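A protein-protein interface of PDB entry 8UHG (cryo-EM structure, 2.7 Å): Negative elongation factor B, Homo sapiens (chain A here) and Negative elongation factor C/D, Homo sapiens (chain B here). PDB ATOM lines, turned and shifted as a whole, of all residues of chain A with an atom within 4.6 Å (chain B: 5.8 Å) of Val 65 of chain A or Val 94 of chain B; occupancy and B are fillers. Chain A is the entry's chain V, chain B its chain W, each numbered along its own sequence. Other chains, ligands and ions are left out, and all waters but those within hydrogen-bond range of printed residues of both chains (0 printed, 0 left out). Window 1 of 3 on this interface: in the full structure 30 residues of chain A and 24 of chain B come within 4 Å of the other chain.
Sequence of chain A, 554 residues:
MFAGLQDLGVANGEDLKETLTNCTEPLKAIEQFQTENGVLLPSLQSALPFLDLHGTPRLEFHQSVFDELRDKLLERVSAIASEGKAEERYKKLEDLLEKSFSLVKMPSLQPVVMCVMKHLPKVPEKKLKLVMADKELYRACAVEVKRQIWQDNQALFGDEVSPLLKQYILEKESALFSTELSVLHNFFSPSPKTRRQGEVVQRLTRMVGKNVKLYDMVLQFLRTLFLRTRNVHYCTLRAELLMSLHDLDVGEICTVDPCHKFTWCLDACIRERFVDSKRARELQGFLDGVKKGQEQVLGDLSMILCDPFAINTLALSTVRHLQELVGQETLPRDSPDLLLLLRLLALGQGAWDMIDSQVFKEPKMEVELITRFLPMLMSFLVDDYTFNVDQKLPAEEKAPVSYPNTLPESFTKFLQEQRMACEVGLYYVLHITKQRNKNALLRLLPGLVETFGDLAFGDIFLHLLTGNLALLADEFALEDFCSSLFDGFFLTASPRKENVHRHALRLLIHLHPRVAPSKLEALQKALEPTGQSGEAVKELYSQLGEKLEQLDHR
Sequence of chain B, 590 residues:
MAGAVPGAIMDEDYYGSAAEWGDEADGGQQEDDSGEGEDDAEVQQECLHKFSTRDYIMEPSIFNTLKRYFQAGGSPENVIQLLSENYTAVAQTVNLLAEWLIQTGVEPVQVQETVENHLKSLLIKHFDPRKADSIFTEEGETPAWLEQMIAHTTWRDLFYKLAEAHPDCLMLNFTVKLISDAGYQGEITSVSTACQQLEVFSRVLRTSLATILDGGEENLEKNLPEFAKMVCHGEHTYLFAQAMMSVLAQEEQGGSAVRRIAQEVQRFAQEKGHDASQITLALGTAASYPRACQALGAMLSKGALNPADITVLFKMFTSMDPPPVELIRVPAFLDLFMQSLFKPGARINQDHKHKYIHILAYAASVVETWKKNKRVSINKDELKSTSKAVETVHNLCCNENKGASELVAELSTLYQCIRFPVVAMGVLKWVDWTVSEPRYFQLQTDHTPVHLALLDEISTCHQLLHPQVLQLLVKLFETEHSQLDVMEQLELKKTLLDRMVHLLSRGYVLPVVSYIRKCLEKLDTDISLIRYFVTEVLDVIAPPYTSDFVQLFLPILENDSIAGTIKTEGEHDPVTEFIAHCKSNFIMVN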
ATOM      1  N   VAL A  39     -15.981 -10.936  -2.829  1.00  0.00           N
ATOM      2  CA  VAL A  39     -16.465  -9.687  -2.247  1.00  0.00           C
ATOM      3  C   VAL A  39     -15.881  -8.548  -3.073  1.00  0.00           C
ATOM      4  O   VAL A  39     -14.659  -8.436  -3.223  1.00  0.00           O
ATOM      5  CB  VAL A  39     -16.087  -9.574  -0.760  1.00  0.00           C
ATOM      6  CG1 VAL A  39     -16.749  -8.355  -0.086  1.00  0.00           C
ATOM      7  CG2 VAL A  39     -16.508 -10.830  -0.012  1.00  0.00           C
ATOM      8  N   PHE A  61     -11.637 -14.418   6.913  1.00  0.00           N
ATOM      9  CA  PHE A  61     -12.049 -13.029   7.064  1.00  0.00           C
ATOM     10  C   PHE A  61     -13.471 -12.843   6.556  1.00  0.00           C
ATOM     11  O   PHE A  61     -14.207 -11.993   7.078  1.00  0.00           O
ATOM     12  CB  PHE A  61     -11.056 -12.070   6.377  1.00  0.00           C
ATOM     13  CG  PHE A  61     -11.237 -11.909   4.885  1.00  0.00           C
ATOM     14  CD1 PHE A  61     -12.061 -10.923   4.358  1.00  0.00           C
ATOM     15  CD2 PHE A  61     -10.511 -12.687   4.011  1.00  0.00           C
ATOM     16  CE1 PHE A  61     -12.203 -10.771   2.998  1.00  0.00           C
ATOM     17  CE2 PHE A  61     -10.647 -12.533   2.648  1.00  0.00           C
ATOM     18  CZ  PHE A  61     -11.489 -11.574   2.145  1.00  0.00           C
ATOM     19  N   HIS A  62     -13.891 -13.643   5.564  1.00  0.00           N
ATOM     20  CA  HIS A  62     -15.303 -13.610   5.194  1.00  0.00           C
ATOM     21  C   HIS A  62     -16.202 -14.015   6.367  1.00  0.00           C
ATOM     22  O   HIS A  62     -17.251 -13.414   6.577  1.00  0.00           O
ATOM     23  CB  HIS A  62     -15.574 -14.504   3.988  1.00  0.00           C
ATOM     24  CG  HIS A  62     -14.918 -14.044   2.723  1.00  0.00           C
ATOM     25  ND1 HIS A  62     -14.308 -14.910   1.840  1.00  0.00           N
ATOM     26  CD2 HIS A  62     -14.802 -12.810   2.177  1.00  0.00           C
ATOM     27  CE1 HIS A  62     -13.827 -14.227   0.817  1.00  0.00           C
ATOM     28  NE2 HIS A  62     -14.113 -12.951   0.998  1.00  0.00           N
ATOM     29  N   GLN A  63     -15.820 -15.033   7.140  1.00  0.00           N
ATOM     30  CA  GLN A  63     -16.640 -15.436   8.282  1.00  0.00           C
ATOM     31  C   GLN A  63     -16.725 -14.322   9.322  1.00  0.00           C
ATOM     32  O   GLN A  63     -17.803 -14.052   9.878  1.00  0.00           O
ATOM     33  CB  GLN A  63     -16.075 -16.717   8.909  1.00  0.00           C
ATOM     34  CG  GLN A  63     -16.509 -16.978  10.363  1.00  0.00           C
ATOM     35  CD  GLN A  63     -16.255 -18.400  10.825  1.00  0.00           C
ATOM     36  OE1 GLN A  63     -15.811 -19.253  10.056  1.00  0.00           O
ATOM     37  NE2 GLN A  63     -16.532 -18.661  12.100  1.00  0.00           N
ATOM     38  N   SER A  64     -15.589 -13.674   9.599  1.00  0.00           N
ATOM     39  CA  SER A  64     -15.580 -12.590  10.581  1.00  0.00           C
ATOM     40  C   SER A  64     -16.505 -11.452  10.152  1.00  0.00           C
ATOM     41  O   SER A  64     -17.392 -11.021  10.912  1.00  0.00           O
ATOM     42  CB  SER A  64     -14.153 -12.077  10.776  1.00  0.00           C
ATOM     43  OG  SER A  64     -13.723 -11.327   9.653  1.00  0.00           O
ATOM     44  N   VAL A  65     -16.338 -10.977   8.915  1.00  0.00           N
ATOM     45  CA  VAL A  65     -17.189  -9.890   8.446  1.00  0.00           C
ATOM     46  C   VAL A  65     -18.627 -10.366   8.270  1.00  0.00           C
ATOM     47  O   VAL A  65     -19.554  -9.570   8.370  1.00  0.00           O
ATOM     48  CB  VAL A  65     -16.637  -9.262   7.152  1.00  0.00           C
ATOM     49  CG1 VAL A  65     -15.189  -8.812   7.342  1.00  0.00           C
ATOM     50  CG2 VAL A  65     -16.754 -10.216   5.989  1.00  0.00           C
ATOM     51  N   PHE A  66     -18.842 -11.654   8.004  1.00  0.00           N
ATOM     52  CA  PHE A  66     -20.199 -12.193   7.932  1.00  0.00           C
ATOM     53  C   PHE A  66     -20.929 -11.997   9.253  1.00  0.00           C
ATOM     54  O   PHE A  66     -22.045 -11.455   9.290  1.00  0.00           O
ATOM     55  CB  PHE A  66     -20.126 -13.677   7.533  1.00  0.00           C
ATOM     56  CG  PHE A  66     -21.251 -14.533   8.055  1.00  0.00           C
ATOM     57  CD1 PHE A  66     -22.432 -14.652   7.350  1.00  0.00           C
ATOM     58  CD2 PHE A  66     -21.099 -15.278   9.217  1.00  0.00           C
ATOM     59  CE1 PHE A  66     -23.462 -15.446   7.816  1.00  0.00           C
ATOM     60  CE2 PHE A  66     -22.124 -16.074   9.688  1.00  0.00           C
ATOM     61  CZ  PHE A  66     -23.305 -16.162   8.982  1.00  0.00           C
ATOM     62  N   ASP A  67     -20.297 -12.413  10.354  1.00  0.00           N
ATOM     63  CA  ASP A  67     -20.912 -12.235  11.667  1.00  0.00           C
ATOM     64  C   ASP A  67     -21.166 -10.756  11.949  1.00  0.00           C
ATOM     65  O   ASP A  67     -22.283 -10.367  12.327  1.00  0.00           O
ATOM     66  CB  ASP A  67     -20.022 -12.849  12.750  1.00  0.00           C
ATOM     67  CG  ASP A  67     -20.806 -13.288  13.973  1.00  0.00           C
ATOM     68  OD1 ASP A  67     -21.851 -12.673  14.269  1.00  0.00           O
ATOM     69  OD2 ASP A  67     -20.373 -14.255  14.638  1.00  0.00           O
ATOM     70  N   GLU A  68     -20.155  -9.914  11.689  1.00  0.00           N
ATOM     71  CA  GLU A  68     -20.288  -8.475  11.931  1.00  0.00           C
ATOM     72  C   GLU A  68     -21.442  -7.870  11.128  1.00  0.00           C
ATOM     73  O   GLU A  68     -22.302  -7.158  11.674  1.00  0.00           O
ATOM     74  CB  GLU A  68     -18.969  -7.782  11.575  1.00  0.00           C
ATOM     75  CG  GLU A  68     -18.863  -6.312  11.980  1.00  0.00           C
ATOM     76  CD  GLU A  68     -18.725  -6.118  13.476  1.00  0.00           C
ATOM     77  OE1 GLU A  68     -17.977  -6.891  14.112  1.00  0.00           O
ATOM     78  OE2 GLU A  68     -19.365  -5.192  14.019  1.00  0.00           O
ATOM     79  N   LEU A  69     -21.491  -8.165   9.832  1.00  0.00           N
ATOM     80  CA  LEU A  69     -22.402  -7.458   8.947  1.00  0.00           C
ATOM     81  C   LEU A  69     -23.842  -7.946   9.086  1.00  0.00           C
ATOM     82  O   LEU A  69     -24.761  -7.130   8.965  1.00  0.00           O
ATOM     83  CB  LEU A  69     -21.906  -7.568   7.500  1.00  0.00           C
ATOM     84  CG  LEU A  69     -20.496  -7.007   7.201  1.00  0.00           C
ATOM     85  CD1 LEU A  69     -19.943  -7.652   5.934  1.00  0.00           C
ATOM     86  CD2 LEU A  69     -20.430  -5.505   7.056  1.00  0.00           C
ATOM     87  N   ALA B  89     -19.648 -21.598   1.370  1.00  0.00           N
ATOM     88  CA  ALA B  89     -19.965 -20.380   0.626  1.00  0.00           C
ATOM     89  C   ALA B  89     -20.079 -19.191   1.575  1.00  0.00           C
ATOM     90  O   ALA B  89     -21.010 -18.388   1.491  1.00  0.00           O
ATOM     91  CB  ALA B  89     -21.237 -20.540  -0.213  1.00  0.00           C
ATOM     92  N   VAL B  90     -19.115 -19.090   2.494  1.00  0.00           N
ATOM     93  CA  VAL B  90     -19.061 -17.958   3.415  1.00  0.00           C
ATOM     94  C   VAL B  90     -18.860 -16.659   2.640  1.00  0.00           C
ATOM     95  O   VAL B  90     -19.386 -15.608   3.025  1.00  0.00           O
ATOM     96  CB  VAL B  90     -17.956 -18.177   4.472  1.00  0.00           C
ATOM     97  CG1 VAL B  90     -17.918 -17.015   5.473  1.00  0.00           C
ATOM     98  CG2 VAL B  90     -18.169 -19.507   5.216  1.00  0.00           C
ATOM     99  N   ALA B  91     -18.112 -16.711   1.534  1.00  0.00           N
ATOM    100  CA  ALA B  91     -17.822 -15.506   0.760  1.00  0.00           C
ATOM    101  C   ALA B  91     -19.082 -14.919   0.130  1.00  0.00           C
ATOM    102  O   ALA B  91     -19.297 -13.701   0.160  1.00  0.00           O
ATOM    103  CB  ALA B  91     -16.781 -15.820  -0.316  1.00  0.00           C
ATOM    104  N   GLN B  92     -19.928 -15.763  -0.463  1.00  0.00           N
ATOM    105  CA  GLN B  92     -21.157 -15.245  -1.063  1.00  0.00           C
ATOM    106  C   GLN B  92     -22.162 -14.835   0.008  1.00  0.00           C
ATOM    107  O   GLN B  92     -22.972 -13.922  -0.210  1.00  0.00           O
ATOM    108  CB  GLN B  92     -21.755 -16.292  -2.007  1.00  0.00           C
ATOM    109  CG  GLN B  92     -22.825 -15.768  -2.962  1.00  0.00           C
ATOM    110  CD  GLN B  92     -22.296 -14.741  -3.948  1.00  0.00           C
ATOM    111  OE1 GLN B  92     -21.279 -14.961  -4.607  1.00  0.00           O
ATOM    112  NE2 GLN B  92     -22.977 -13.604  -4.042  1.00  0.00           N
ATOM    113  N   THR B  93     -22.122 -15.495   1.166  1.00  0.00           N
ATOM    114  CA  THR B  93     -22.850 -15.011   2.333  1.00  0.00           C
ATOM    115  C   THR B  93     -22.430 -13.581   2.666  1.00  0.00           C
ATOM    116  O   THR B  93     -23.270 -12.716   2.946  1.00  0.00           O
ATOM    117  CB  THR B  93     -22.611 -15.962   3.508  1.00  0.00           C
ATOM    118  OG1 THR B  93     -22.482 -17.302   3.015  1.00  0.00           O
ATOM    119  CG2 THR B  93     -23.770 -15.935   4.485  1.00  0.00           C
ATOM    120  N   VAL B  94     -21.123 -13.310   2.606  1.00  0.00           N
ATOM    121  CA  VAL B  94     -20.632 -11.954   2.840  1.00  0.00           C
ATOM    122  C   VAL B  94     -21.099 -11.007   1.745  1.00  0.00           C
ATOM    123  O   VAL B  94     -21.348  -9.828   2.006  1.00  0.00           O
ATOM    124  CB  VAL B  94     -19.099 -11.944   2.961  1.00  0.00           C
ATOM    125  CG1 VAL B  94     -18.549 -10.508   2.893  1.00  0.00           C
ATOM    126  CG2 VAL B  94     -18.706 -12.573   4.237  1.00  0.00           C
ATOM    127  N   ASN B  95     -21.143 -11.482   0.499  1.00  0.00           N
ATOM    128  CA  ASN B  95     -21.662 -10.650  -0.587  1.00  0.00           C
ATOM    129  C   ASN B  95     -23.076 -10.185  -0.269  1.00  0.00           C
ATOM    130  O   ASN B  95     -23.374  -8.982  -0.290  1.00  0.00           O
ATOM    131  CB  ASN B  95     -21.653 -11.423  -1.909  1.00  0.00           C
ATOM    132  CG  ASN B  95     -20.298 -11.438  -2.570  1.00  0.00           C
ATOM    133  OD1 ASN B  95     -19.636 -12.472  -2.632  1.00  0.00           O
ATOM    134  ND2 ASN B  95     -19.885 -10.290  -3.090  1.00  0.00           N
ATOM    135  N   LEU B  96     -23.936 -11.139   0.096  1.00  0.00           N
ATOM    136  CA  LEU B  96     -25.321 -10.838   0.447  1.00  0.00           C
ATOM    137  C   LEU B  96     -25.396  -9.855   1.615  1.00  0.00           C
ATOM    138  O   LEU B  96     -26.122  -8.854   1.565  1.00  0.00           O
ATOM    139  CB  LEU B  96     -26.047 -12.141   0.790  1.00  0.00           C
ATOM    140  CG  LEU B  96     -26.147 -13.205  -0.312  1.00  0.00           C
ATOM    141  CD1 LEU B  96     -26.112 -14.622   0.256  1.00  0.00           C
ATOM    142  CD2 LEU B  96     -27.415 -13.007  -1.122  1.00  0.00           C
ATOM    143  N   LEU B  97     -24.610 -10.103   2.660  1.00  0.00           N
ATOM    144  CA  LEU B  97     -24.710  -9.291   3.871  1.00  0.00           C
ATOM    145  C   LEU B  97     -24.174  -7.879   3.655  1.00  0.00           C
ATOM    146  O   LEU B  97     -24.799  -6.896   4.073  1.00  0.00           O
ATOM    147  CB  LEU B  97     -23.955  -9.973   5.003  1.00  0.00           C
ATOM    148  CG  LEU B  97     -24.654 -11.051   5.839  1.00  0.00           C
ATOM    149  CD1 LEU B  97     -25.351 -12.195   5.082  1.00  0.00           C
ATOM    150  CD2 LEU B  97     -23.591 -11.608   6.733  1.00  0.00           C
ATOM    151  N   ALA B  98     -22.995  -7.761   3.040  1.00  0.00           N
ATOM    152  CA  ALA B  98     -22.395  -6.453   2.813  1.00  0.00           C
ATOM    153  C   ALA B  98     -23.245  -5.619   1.864  1.00  0.00           C
ATOM    154  O   ALA B  98     -23.460  -4.420   2.094  1.00  0.00           O
ATOM    155  CB  ALA B  98     -20.979  -6.623   2.265  1.00  0.00           C
ATOM    156  N   GLU B  99     -23.747  -6.234   0.787  1.00  0.00           N
ATOM    157  CA  GLU B  99     -24.599  -5.472  -0.112  1.00  0.00           C
ATOM    158  C   GLU B  99     -25.933  -5.129   0.532  1.00  0.00           C
ATOM    159  O   GLU B  99     -26.545  -4.131   0.141  1.00  0.00           O
ATOM    160  CB  GLU B  99     -24.808  -6.227  -1.431  1.00  0.00           C
ATOM    161  CG  GLU B  99     -25.815  -7.366  -1.402  1.00  0.00           C
ATOM    162  CD  GLU B  99     -25.735  -8.240  -2.636  1.00  0.00           C
ATOM    163  OE1 GLU B  99     -25.141  -7.797  -3.641  1.00  0.00           O
ATOM    164  OE2 GLU B  99     -26.260  -9.373  -2.598  1.00  0.00           O
ATOM    165  N   VAL B 115     -13.710  -3.490   8.771  1.00  0.00           N
ATOM    166  CA  VAL B 115     -12.900  -4.563   8.200  1.00  0.00           C
ATOM    167  C   VAL B 115     -11.416  -4.264   8.373  1.00  0.00           C
ATOM    168  O   VAL B 115     -10.626  -5.157   8.715  1.00  0.00           O
ATOM    169  CB  VAL B 115     -13.265  -4.782   6.718  1.00  0.00           C
ATOM    170  CG1 VAL B 115     -12.296  -5.774   6.063  1.00  0.00           C
ATOM    171  CG2 VAL B 115     -14.698  -5.285   6.598  1.00  0.00           C
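CG2 of Val 39 of chain A touches CG1 of Val 94 of chain B, at 3.6 Å.
Val 39 of chain A touches Asn 95 of chain B.
His 62 of chain A touches Val 90 of chain B (C to CG1, 3.6 Å).
ND1 of His 62 of chain A touches CB of Ala 91 of chain B (3.4 Å).
Val 94 of chain B touches His 62 of chain A.
Gln 63 of chain A touches Val 90 of chain B.
Val 65 of chain A touches Val 94 of chain B (CG2 to CG2, 3.5 Å).
Val 115 of chain B touches Val 65 of chain A (CG2 to CG1, 3.6 Å).
CG2 of Thr 93 of chain B touches CE1 of Phe 66 of chain A, at 3.4 Å.
CB of Ala 98 of chain B touches CD1 of Leu 69 of chain A, 3.9 Å away.
Printed residues of chain B within 4 Å of Val 39 of chain A: Val 94 and Asn 95.
Of chain B, only Val 94 and Val 115 come within 4 Å of Val 65 of chain A.
Printed residues of chain A within 4 Å of Thr 93 of chain B: Phe 66 (3.4 Å).
The nearest residue of chain B that does not touch Val 65 of chain A is Leu 97 of chain B (4.8 Å).
The nearest printed residue of chain A that does not touch Ala 91 of chain B is Val 39 of chain A (4.01 Å).
Of the 10 printed residues of chain A, 6 touch a printed residue of chain B.
Hydrophobic or aromatic side chains of chain A that line the printed part of chain B: Val 39, His 62, Val 65, Phe 66 and Leu 69.
Along chain A the printed residues that touch a printed residue of chain B span positions 39 to 69.
Of the 12 printed residues of chain B, 8 touch a printed residue of chain A.
The backbone carbonyl oxygen of Ala 91 of chain B sits close to the side-chain amide oxygen of Asn 95 of chain B (3.1 Å).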
